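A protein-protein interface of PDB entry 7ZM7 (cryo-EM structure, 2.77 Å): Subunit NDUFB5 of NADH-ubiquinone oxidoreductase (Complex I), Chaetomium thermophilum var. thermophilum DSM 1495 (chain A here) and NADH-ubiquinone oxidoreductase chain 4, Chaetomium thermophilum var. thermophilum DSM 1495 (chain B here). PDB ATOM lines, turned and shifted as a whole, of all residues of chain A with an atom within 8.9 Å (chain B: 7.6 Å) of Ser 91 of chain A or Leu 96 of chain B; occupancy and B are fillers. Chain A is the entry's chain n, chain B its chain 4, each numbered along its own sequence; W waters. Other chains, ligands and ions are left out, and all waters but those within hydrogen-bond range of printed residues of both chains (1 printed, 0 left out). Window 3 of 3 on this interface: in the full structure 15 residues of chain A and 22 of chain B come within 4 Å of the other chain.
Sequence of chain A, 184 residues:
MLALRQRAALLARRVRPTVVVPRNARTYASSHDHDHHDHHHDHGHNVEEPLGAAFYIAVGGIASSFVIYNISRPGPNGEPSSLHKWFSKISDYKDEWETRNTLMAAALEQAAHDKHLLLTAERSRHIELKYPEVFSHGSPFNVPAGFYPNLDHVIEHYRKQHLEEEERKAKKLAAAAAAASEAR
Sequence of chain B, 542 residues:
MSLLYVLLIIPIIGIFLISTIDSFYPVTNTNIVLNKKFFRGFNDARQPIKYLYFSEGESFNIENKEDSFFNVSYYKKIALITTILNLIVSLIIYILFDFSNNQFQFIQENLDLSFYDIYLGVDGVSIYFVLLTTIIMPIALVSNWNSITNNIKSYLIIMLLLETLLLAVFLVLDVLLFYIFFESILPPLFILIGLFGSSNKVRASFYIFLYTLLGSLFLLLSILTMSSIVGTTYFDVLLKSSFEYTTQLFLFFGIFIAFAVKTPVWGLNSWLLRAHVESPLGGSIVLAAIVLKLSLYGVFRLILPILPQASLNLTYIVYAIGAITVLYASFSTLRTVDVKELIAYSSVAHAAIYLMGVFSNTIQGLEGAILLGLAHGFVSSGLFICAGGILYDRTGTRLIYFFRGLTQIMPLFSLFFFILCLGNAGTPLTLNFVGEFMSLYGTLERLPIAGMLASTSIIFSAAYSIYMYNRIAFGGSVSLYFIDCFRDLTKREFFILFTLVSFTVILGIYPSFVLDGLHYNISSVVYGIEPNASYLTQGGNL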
ATOM      1  N   HIS A  84     -11.653  -3.081  18.030  1.00  0.00           N
ATOM      2  CA  HIS A  84     -10.549  -4.068  17.948  1.00  0.00           C
ATOM      3  C   HIS A  84     -11.120  -5.487  18.080  1.00  0.00           C
ATOM      4  O   HIS A  84     -10.703  -6.357  17.291  1.00  0.00           O
ATOM      5  CB  HIS A  84      -9.487  -3.761  19.007  1.00  0.00           C
ATOM      6  CG  HIS A  84      -8.660  -2.557  18.708  1.00  0.00           C
ATOM      7  ND1 HIS A  84      -7.468  -2.636  18.019  1.00  0.00           N
ATOM      8  CD2 HIS A  84      -8.836  -1.256  19.013  1.00  0.00           C
ATOM      9  CE1 HIS A  84      -6.949  -1.433  17.904  1.00  0.00           C
ATOM     10  NE2 HIS A  84      -7.771  -0.568  18.503  1.00  0.00           N
ATOM     11  N   LYS A  85     -12.025  -5.714  19.039  1.00  0.00           N
ATOM     12  CA  LYS A  85     -12.609  -7.039  19.186  1.00  0.00           C
ATOM     13  C   LYS A  85     -13.402  -7.416  17.949  1.00  0.00           C
ATOM     14  O   LYS A  85     -13.435  -8.586  17.555  1.00  0.00           O
ATOM     15  CB  LYS A  85     -13.485  -7.098  20.434  1.00  0.00           C
ATOM     16  CG  LYS A  85     -12.716  -7.424  21.701  1.00  0.00           C
ATOM     17  CD  LYS A  85     -13.648  -7.625  22.879  1.00  0.00           C
ATOM     18  CE  LYS A  85     -12.868  -7.966  24.137  1.00  0.00           C
ATOM     19  NZ  LYS A  85     -13.757  -8.093  25.323  1.00  0.00           N
ATOM     20  N   TRP A  86     -14.048  -6.436  17.320  1.00  0.00           N
ATOM     21  CA  TRP A  86     -14.755  -6.714  16.081  1.00  0.00           C
ATOM     22  C   TRP A  86     -13.790  -7.106  14.976  1.00  0.00           C
ATOM     23  O   TRP A  86     -14.043  -8.062  14.234  1.00  0.00           O
ATOM     24  CB  TRP A  86     -15.577  -5.506  15.650  1.00  0.00           C
ATOM     25  CG  TRP A  86     -16.473  -5.833  14.499  1.00  0.00           C
ATOM     26  CD1 TRP A  86     -17.528  -6.685  14.512  1.00  0.00           C
ATOM     27  CD2 TRP A  86     -16.380  -5.331  13.164  1.00  0.00           C
ATOM     28  NE1 TRP A  86     -18.108  -6.742  13.276  1.00  0.00           N
ATOM     29  CE2 TRP A  86     -17.422  -5.917  12.428  1.00  0.00           C
ATOM     30  CE3 TRP A  86     -15.521  -4.438  12.521  1.00  0.00           C
ATOM     31  CZ2 TRP A  86     -17.629  -5.644  11.081  1.00  0.00           C
ATOM     32  CZ3 TRP A  86     -15.733  -4.166  11.184  1.00  0.00           C
ATOM     33  CH2 TRP A  86     -16.776  -4.766  10.481  1.00  0.00           C
ATOM     34  N   PHE A  87     -12.679  -6.375  14.846  1.00  0.00           N
ATOM     35  CA  PHE A  87     -11.763  -6.634  13.742  1.00  0.00           C
ATOM     36  C   PHE A  87     -11.162  -8.020  13.823  1.00  0.00           C
ATOM     37  O   PHE A  87     -11.204  -8.774  12.848  1.00  0.00           O
ATOM     38  CB  PHE A  87     -10.665  -5.579  13.690  1.00  0.00           C
ATOM     39  CG  PHE A  87     -11.004  -4.408  12.844  1.00  0.00           C
ATOM     40  CD1 PHE A  87     -10.711  -4.425  11.501  1.00  0.00           C
ATOM     41  CD2 PHE A  87     -11.637  -3.311  13.365  1.00  0.00           C
ATOM     42  CE1 PHE A  87     -11.015  -3.359  10.695  1.00  0.00           C
ATOM     43  CE2 PHE A  87     -11.947  -2.237  12.563  1.00  0.00           C
ATOM     44  CZ  PHE A  87     -11.630  -2.264  11.225  1.00  0.00           C
ATOM     45  N   SER A  88     -10.614  -8.389  14.974  1.00  0.00           N
ATOM     46  CA  SER A  88     -10.001  -9.706  15.078  1.00  0.00           C
ATOM     47  C   SER A  88     -11.034 -10.808  14.910  1.00  0.00           C
ATOM     48  O   SER A  88     -10.683 -11.936  14.552  1.00  0.00           O
ATOM     49  CB  SER A  88      -9.278  -9.847  16.412  1.00  0.00           C
ATOM     50  OG  SER A  88     -10.198  -9.801  17.488  1.00  0.00           O
ATOM     51  N   LYS A  89     -12.307 -10.504  15.159  1.00  0.00           N
ATOM     52  CA  LYS A  89     -13.352 -11.506  14.991  1.00  0.00           C
ATOM     53  C   LYS A  89     -13.598 -11.817  13.521  1.00  0.00           C
ATOM     54  O   LYS A  89     -13.658 -12.989  13.132  1.00  0.00           O
ATOM     55  CB  LYS A  89     -14.644 -11.038  15.654  1.00  0.00           C
ATOM     56  CG  LYS A  89     -15.807 -11.981  15.420  1.00  0.00           C
ATOM     57  CD  LYS A  89     -17.107 -11.422  15.962  1.00  0.00           C
ATOM     58  CE  LYS A  89     -18.274 -12.319  15.596  1.00  0.00           C
ATOM     59  NZ  LYS A  89     -19.574 -11.736  16.018  1.00  0.00           N
ATOM     60  N   ILE A  90     -13.745 -10.787  12.687  1.00  0.00           N
ATOM     61  CA  ILE A  90     -14.171 -11.027  11.312  1.00  0.00           C
ATOM     62  C   ILE A  90     -13.109 -11.802  10.551  1.00  0.00           C
ATOM     63  O   ILE A  90     -13.423 -12.696   9.757  1.00  0.00           O
ATOM     64  CB  ILE A  90     -14.532  -9.710  10.595  1.00  0.00           C
ATOM     65  CG1 ILE A  90     -13.396  -8.692  10.678  1.00  0.00           C
ATOM     66  CG2 ILE A  90     -15.805  -9.118  11.167  1.00  0.00           C
ATOM     67  CD1 ILE A  90     -13.619  -7.480   9.845  1.00  0.00           C
ATOM     68  N   SER A  91     -11.846 -11.475  10.769  1.00  0.00           N
ATOM     69  CA  SER A  91     -10.744 -12.114  10.055  1.00  0.00           C
ATOM     70  C   SER A  91     -10.096 -13.209  10.901  1.00  0.00           C
ATOM     71  O   SER A  91      -8.894 -13.215  11.122  1.00  0.00           O
ATOM     72  CB  SER A  91      -9.729 -11.060   9.644  1.00  0.00           C
ATOM     73  OG  SER A  91      -9.283 -10.344  10.784  1.00  0.00           O
ATOM     74  N   ASP A  92     -10.897 -14.166  11.367  1.00  0.00           N
ATOM     75  CA  ASP A  92     -10.340 -15.201  12.237  1.00  0.00           C
ATOM     76  C   ASP A  92      -9.698 -16.316  11.418  1.00  0.00           C
ATOM     77  O   ASP A  92      -8.475 -16.488  11.441  1.00  0.00           O
ATOM     78  CB  ASP A  92     -11.417 -15.754  13.179  1.00  0.00           C
ATOM     79  CG  ASP A  92     -12.652 -16.236  12.446  1.00  0.00           C
ATOM     80  OD1 ASP A  92     -12.673 -16.163  11.198  1.00  0.00           O
ATOM     81  OD2 ASP A  92     -13.598 -16.699  13.117  1.00  0.00           O
ATOM     82  N   TYR A  93     -10.508 -17.058  10.666  1.00  0.00           N
ATOM     83  CA  TYR A  93     -10.033 -18.130   9.794  1.00  0.00           C
ATOM     84  C   TYR A  93      -9.052 -19.041  10.526  1.00  0.00           C
ATOM     85  O   TYR A  93      -7.976 -19.379  10.021  1.00  0.00           O
ATOM     86  CB  TYR A  93      -9.405 -17.546   8.535  1.00  0.00           C
ATOM     87  CG  TYR A  93     -10.234 -16.466   7.902  1.00  0.00           C
ATOM     88  CD1 TYR A  93     -11.566 -16.674   7.624  1.00  0.00           C
ATOM     89  CD2 TYR A  93      -9.688 -15.235   7.603  1.00  0.00           C
ATOM     90  CE1 TYR A  93     -12.329 -15.697   7.052  1.00  0.00           C
ATOM     91  CE2 TYR A  93     -10.437 -14.248   7.034  1.00  0.00           C
ATOM     92  CZ  TYR A  93     -11.763 -14.484   6.758  1.00  0.00           C
ATOM     93  OH  TYR A  93     -12.532 -13.500   6.182  1.00  0.00           O
ATOM     94  N   LYS A  94      -9.451 -19.453  11.734  1.00  0.00           N
ATOM     95  CA  LYS A  94      -8.528 -20.125  12.646  1.00  0.00           C
ATOM     96  C   LYS A  94      -7.881 -21.336  11.989  1.00  0.00           C
ATOM     97  O   LYS A  94      -6.670 -21.551  12.106  1.00  0.00           O
ATOM     98  CB  LYS A  94      -9.260 -20.531  13.928  1.00  0.00           C
ATOM     99  CG  LYS A  94     -10.530 -21.335  13.701  1.00  0.00           C
ATOM    100  CD  LYS A  94     -11.319 -21.512  14.984  1.00  0.00           C
ATOM    101  CE  LYS A  94     -12.272 -20.354  15.211  1.00  0.00           C
ATOM    102  NZ  LYS A  94     -13.359 -20.334  14.194  1.00  0.00           N
ATOM    103  N   GLU A  96      -9.568 -22.326   8.758  1.00  0.00           N
ATOM    104  CA  GLU A  96     -10.348 -22.411   7.533  1.00  0.00           C
ATOM    105  C   GLU A  96      -9.472 -22.399   6.293  1.00  0.00           C
ATOM    106  O   GLU A  96      -9.815 -23.039   5.300  1.00  0.00           O
ATOM    107  CB  GLU A  96     -11.368 -21.280   7.496  1.00  0.00           C
ATOM    108  CG  GLU A  96     -12.301 -21.315   6.309  1.00  0.00           C
ATOM    109  CD  GLU A  96     -11.907 -20.305   5.265  1.00  0.00           C
ATOM    110  OE1 GLU A  96     -11.304 -19.282   5.641  1.00  0.00           O
ATOM    111  OE2 GLU A  96     -12.196 -20.523   4.076  1.00  0.00           O
ATOM    112  N   TRP A  97      -8.352 -21.687   6.318  1.00  0.00           N
ATOM    113  CA  TRP A  97      -7.451 -21.774   5.144  1.00  0.00           C
ATOM    114  C   TRP A  97      -6.727 -23.123   5.159  1.00  0.00           C
ATOM    115  O   TRP A  97      -6.610 -23.740   4.093  1.00  0.00           O
ATOM    116  CB  TRP A  97      -6.475 -20.594   5.076  1.00  0.00           C
ATOM    117  CG  TRP A  97      -7.102 -19.234   5.106  1.00  0.00           C
ATOM    118  CD1 TRP A  97      -6.732 -18.190   5.901  1.00  0.00           C
ATOM    119  CD2 TRP A  97      -8.198 -18.757   4.303  1.00  0.00           C
ATOM    120  NE1 TRP A  97      -7.521 -17.100   5.652  1.00  0.00           N
ATOM    121  CE2 TRP A  97      -8.431 -17.418   4.680  1.00  0.00           C
ATOM    122  CE3 TRP A  97      -9.006 -19.323   3.311  1.00  0.00           C
ATOM    123  CZ2 TRP A  97      -9.437 -16.646   4.105  1.00  0.00           C
ATOM    124  CZ3 TRP A  97     -10.000 -18.560   2.744  1.00  0.00           C
ATOM    125  CH2 TRP A  97     -10.217 -17.243   3.144  1.00  0.00           C
ATOM    126  N   LEU B   3     -13.221 -14.057  -2.836  1.00  0.00           N
ATOM    127  CA  LEU B   3     -13.045 -12.621  -2.944  1.00  0.00           C
ATOM    128  C   LEU B   3     -11.913 -12.258  -3.888  1.00  0.00           C
ATOM    129  O   LEU B   3     -11.809 -11.100  -4.297  1.00  0.00           O
ATOM    130  CB  LEU B   3     -12.809 -12.030  -1.551  1.00  0.00           C
ATOM    131  CG  LEU B   3     -12.667 -10.523  -1.391  1.00  0.00           C
ATOM    132  CD1 LEU B   3     -13.936  -9.838  -1.809  1.00  0.00           C
ATOM    133  CD2 LEU B   3     -12.349 -10.197   0.030  1.00  0.00           C
ATOM    134  N   SER B  90      -9.281  -4.405  -3.047  1.00  0.00           N
ATOM    135  CA  SER B  90      -7.939  -4.884  -2.762  1.00  0.00           C
ATOM    136  C   SER B  90      -7.474  -4.455  -1.379  1.00  0.00           C
ATOM    137  O   SER B  90      -6.678  -5.151  -0.744  1.00  0.00           O
ATOM    138  CB  SER B  90      -6.982  -4.393  -3.836  1.00  0.00           C
ATOM    139  OG  SER B  90      -6.604  -3.058  -3.592  1.00  0.00           O
ATOM    140  N   LEU B  91      -7.936  -3.298  -0.904  1.00  0.00           N
ATOM    141  CA  LEU B  91      -7.637  -2.882   0.459  1.00  0.00           C
ATOM    142  C   LEU B  91      -8.474  -3.650   1.473  1.00  0.00           C
ATOM    143  O   LEU B  91      -8.043  -3.845   2.610  1.00  0.00           O
ATOM    144  CB  LEU B  91      -7.854  -1.381   0.602  1.00  0.00           C
ATOM    145  CG  LEU B  91      -7.000  -0.506  -0.309  1.00  0.00           C
ATOM    146  CD1 LEU B  91      -7.654   0.845  -0.530  1.00  0.00           C
ATOM    147  CD2 LEU B  91      -5.575  -0.343   0.207  1.00  0.00           C
ATOM    148  N   ILE B  92      -9.666  -4.085   1.086  1.00  0.00           N
ATOM    149  CA  ILE B  92     -10.443  -4.975   1.938  1.00  0.00           C
ATOM    150  C   ILE B  92      -9.728  -6.309   2.099  1.00  0.00           C
ATOM    151  O   ILE B  92      -9.659  -6.863   3.201  1.00  0.00           O
ATOM    152  CB  ILE B  92     -11.861  -5.145   1.363  1.00  0.00           C
ATOM    153  CG1 ILE B  92     -12.598  -3.811   1.433  1.00  0.00           C
ATOM    154  CG2 ILE B  92     -12.612  -6.215   2.101  1.00  0.00           C
ATOM    155  CD1 ILE B  92     -13.605  -3.632   0.373  1.00  0.00           C
ATOM    156  N   ILE B  93      -9.178  -6.838   1.007  1.00  0.00           N
ATOM    157  CA  ILE B  93      -8.374  -8.050   1.080  1.00  0.00           C
ATOM    158  C   ILE B  93      -7.167  -7.840   1.981  1.00  0.00           C
ATOM    159  O   ILE B  93      -6.743  -8.755   2.690  1.00  0.00           O
ATOM    160  CB  ILE B  93      -7.958  -8.501  -0.333  1.00  0.00           C
ATOM    161  CG1 ILE B  93      -9.172  -8.987  -1.102  1.00  0.00           C
ATOM    162  CG2 ILE B  93      -6.930  -9.614  -0.275  1.00  0.00           C
ATOM    163  CD1 ILE B  93      -8.964  -9.046  -2.548  1.00  0.00           C
ATOM    164  N   TYR B  94      -6.597  -6.641   1.979  1.00  0.00           N
ATOM    165  CA  TYR B  94      -5.381  -6.431   2.750  1.00  0.00           C
ATOM    166  C   TYR B  94      -5.664  -6.285   4.240  1.00  0.00           C
ATOM    167  O   TYR B  94      -4.816  -6.639   5.059  1.00  0.00           O
ATOM    168  CB  TYR B  94      -4.626  -5.221   2.221  1.00  0.00           C
ATOM    169  CG  TYR B  94      -3.364  -4.958   2.976  1.00  0.00           C
ATOM    170  CD1 TYR B  94      -2.215  -5.683   2.710  1.00  0.00           C
ATOM    171  CD2 TYR B  94      -3.316  -4.010   3.971  1.00  0.00           C
ATOM    172  CE1 TYR B  94      -1.067  -5.448   3.388  1.00  0.00           C
ATOM    173  CE2 TYR B  94      -2.172  -3.786   4.668  1.00  0.00           C
ATOM    174  CZ  TYR B  94      -1.051  -4.506   4.374  1.00  0.00           C
ATOM    175  OH  TYR B  94       0.092  -4.256   5.073  1.00  0.00           O
ATOM    176  N   ILE B  95      -6.830  -5.757   4.614  1.00  0.00           N
ATOM    177  CA  ILE B  95      -7.203  -5.690   6.025  1.00  0.00           C
ATOM    178  C   ILE B  95      -7.409  -7.088   6.594  1.00  0.00           C
ATOM    179  O   ILE B  95      -7.143  -7.338   7.774  1.00  0.00           O
ATOM    180  CB  ILE B  95      -8.465  -4.829   6.221  1.00  0.00           C
ATOM    181  CG1 ILE B  95      -8.259  -3.408   5.715  1.00  0.00           C
ATOM    182  CG2 ILE B  95      -8.838  -4.777   7.670  1.00  0.00           C
ATOM    183  CD1 ILE B  95      -7.157  -2.636   6.419  1.00  0.00           C
ATOM    184  N   LEU B  96      -7.928  -8.002   5.786  1.00  0.00           N
ATOM    185  CA  LEU B  96      -8.236  -9.342   6.251  1.00  0.00           C
ATOM    186  C   LEU B  96      -7.073 -10.295   6.085  1.00  0.00           C
ATOM    187  O   LEU B  96      -7.208 -11.474   6.409  1.00  0.00           O
ATOM    188  CB  LEU B  96      -9.470  -9.890   5.527  1.00  0.00           C
ATOM    189  CG  LEU B  96     -10.709  -9.002   5.675  1.00  0.00           C
ATOM    190  CD1 LEU B  96     -11.903  -9.577   4.977  1.00  0.00           C
ATOM    191  CD2 LEU B  96     -11.021  -8.740   7.128  1.00  0.00           C
ATOM    192  N   PHE B  97      -5.938  -9.812   5.614  1.00  0.00           N
ATOM    193  CA  PHE B  97      -4.778 -10.651   5.421  1.00  0.00           C
ATOM    194  C   PHE B  97      -4.193 -11.072   6.765  1.00  0.00           C
ATOM    195  O   PHE B  97      -4.429 -10.444   7.794  1.00  0.00           O
ATOM    196  CB  PHE B  97      -3.740  -9.912   4.587  1.00  0.00           C
ATOM    197  CG  PHE B  97      -2.713 -10.803   4.000  1.00  0.00           C
ATOM    198  CD1 PHE B  97      -3.050 -11.688   3.010  1.00  0.00           C
ATOM    199  CD2 PHE B  97      -1.416 -10.776   4.453  1.00  0.00           C
ATOM    200  CE1 PHE B  97      -2.123 -12.517   2.484  1.00  0.00           C
ATOM    201  CE2 PHE B  97      -0.498 -11.604   3.925  1.00  0.00           C
ATOM    202  CZ  PHE B  97      -0.855 -12.479   2.940  1.00  0.00           C
ATOM    203  N   ASP B  98      -3.442 -12.170   6.750  1.00  0.00           N
ATOM    204  CA  ASP B  98      -2.776 -12.697   7.938  1.00  0.00           C
ATOM    205  C   ASP B  98      -1.278 -12.675   7.686  1.00  0.00           C
ATOM    206  O   ASP B  98      -0.770 -13.455   6.879  1.00  0.00           O
ATOM    207  CB  ASP B  98      -3.255 -14.109   8.255  1.00  0.00           C
ATOM    208  CG  ASP B  98      -2.788 -14.595   9.601  1.00  0.00           C
ATOM    209  OD1 ASP B  98      -1.612 -14.963   9.738  1.00  0.00           O
ATOM    210  OD2 ASP B  98      -3.609 -14.623  10.530  1.00  0.00           O
ATOM    211  N   PHE B  99      -0.571 -11.804   8.389  1.00  0.00           N
ATOM    212  CA  PHE B  99       0.810 -11.490   8.053  1.00  0.00           C
ATOM    213  C   PHE B  99       1.793 -12.607   8.354  1.00  0.00           C
ATOM    214  O   PHE B  99       2.943 -12.504   7.927  1.00  0.00           O
ATOM    215  CB  PHE B  99       1.273 -10.236   8.793  1.00  0.00           C
ATOM    216  CG  PHE B  99       0.788  -8.958   8.205  1.00  0.00           C
ATOM    217  CD1 PHE B  99       0.238  -8.926   6.944  1.00  0.00           C
ATOM    218  CD2 PHE B  99       0.915  -7.780   8.901  1.00  0.00           C
ATOM    219  CE1 PHE B  99      -0.190  -7.755   6.393  1.00  0.00           C
ATOM    220  CE2 PHE B  99       0.490  -6.606   8.356  1.00  0.00           C
ATOM    221  CZ  PHE B  99      -0.068  -6.595   7.094  1.00  0.00           C
ATOM    222  N   GLN B 105      -4.108 -17.914   1.285  1.00  0.00           N
ATOM    223  CA  GLN B 105      -5.308 -17.322   1.917  1.00  0.00           C
ATOM    224  C   GLN B 105      -6.307 -16.897   0.842  1.00  0.00           C
ATOM    225  O   GLN B 105      -5.881 -16.731  -0.302  1.00  0.00           O
ATOM    226  CB  GLN B 105      -4.895 -16.132   2.782  1.00  0.00           C
ATOM    227  CG  GLN B 105      -3.906 -16.472   3.881  1.00  0.00           C
ATOM    228  CD  GLN B 105      -3.438 -15.224   4.587  1.00  0.00           C
ATOM    229  OE1 GLN B 105      -4.201 -14.287   4.791  1.00  0.00           O
ATOM    230  NE2 GLN B 105      -2.169 -15.203   4.957  1.00  0.00           N
ATOM    231  N   PHE B 106      -7.584 -16.772   1.200  1.00  0.00           N
ATOM    232  CA  PHE B 106      -8.673 -16.344   0.278  1.00  0.00           C
ATOM    233  C   PHE B 106      -8.847 -17.362  -0.846  1.00  0.00           C
ATOM    234  O   PHE B 106      -9.259 -16.991  -1.951  1.00  0.00           O
ATOM    235  CB  PHE B 106      -8.559 -14.860  -0.066  1.00  0.00           C
ATOM    236  CG  PHE B 106      -8.566 -13.938   1.124  1.00  0.00           C
ATOM    237  CD1 PHE B 106      -9.758 -13.504   1.676  1.00  0.00           C
ATOM    238  CD2 PHE B 106      -7.380 -13.502   1.691  1.00  0.00           C
ATOM    239  CE1 PHE B 106      -9.759 -12.660   2.772  1.00  0.00           C
ATOM    240  CE2 PHE B 106      -7.381 -12.656   2.786  1.00  0.00           C
ATOM    241  CZ  PHE B 106      -8.572 -12.240   3.325  1.00  0.00           C
ATOM    242  N   VAL B 122      -3.778 -15.821  -2.257  1.00  0.00           N
ATOM    243  CA  VAL B 122      -2.984 -14.638  -1.977  1.00  0.00           C
ATOM    244  C   VAL B 122      -1.995 -14.979  -0.877  1.00  0.00           C
ATOM    245  O   VAL B 122      -2.330 -15.672   0.088  1.00  0.00           O
ATOM    246  CB  VAL B 122      -3.859 -13.424  -1.593  1.00  0.00           C
ATOM    247  CG1 VAL B 122      -4.653 -13.706  -0.356  1.00  0.00           C
ATOM    248  CG2 VAL B 122      -3.009 -12.198  -1.382  1.00  0.00           C
HETATM  249  O   HOH W   1      -6.445 -14.142   6.449  1.00  0.00           O
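O of Asp 98 of chain B sits at hydrogen-bond distance from NE2 of Gln 105 of chain B.
N of Val 122 of chain B sits at hydrogen-bond distance from O of Gln 105 of chain B.
O of Phe 87 of chain A sits at hydrogen-bond distance from OG of Ser 91 of chain A (3.2 Å).
Phe 87 of chain A touches Ile 95 of chain B.
Ile 90 of chain A touches Leu 96 of chain B (CD1 to CD2, 3.96 Å).
Ser 91 of chain A touches Leu 96 of chain B.
CG of Gln 105 of chain B touches CD1 of Trp 97 of chain A, 3.9 Å away.
Phe 106 of chain B touches Trp 97 of chain A.
Of the printed residues of chain B, Phe 87 of chain A touches Ile 95.
Ser 91 of chain A touches just one residue of chain B: Leu 96 (3.7 Å).
Of the printed residues of chain B, Trp 97 of chain A touches Gln 105 (3.9 Å) and Phe 106 (3.3 Å).
Of the printed residues of chain A, Ile 95 of chain B touches Phe 87 (3.99 Å).
Of chain A, only Ile 90 (3.96 Å) and Ser 91 (3.7 Å) come within 4 Å of Leu 96 of chain B.
Printed residues of chain A within 4 Å of Gln 105 of chain B: Trp 97.
Of the printed residues of chain A, Phe 106 of chain B touches Trp 97 (3.3 Å).
Hydrophobic or aromatic side chains of chain B that line the printed part of chain A: Ile 95, Leu 96 and Phe 106.
Hydrophobic or aromatic side chains of chain A that line the printed part of chain B: Phe 87, Ile 90 and Trp 97.
Among the printed residues, 5 pairs touch across the chains.
Among the printed residues, no Asp or Glu carboxylate lies within 4 Å of a Lys or Arg side-chain nitrogen of the other chain.
Water W1 lies within hydrogen-bond range of the backbone carbonyl oxygen (O) of Leu 96 of chain B (2.8 Å), the side-chain amide oxygen (OE1) of Gln 105 of chain B (2.8 Å) and the indole nitrogen (NE1) of Trp 97 of chain A (3.2 Å).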
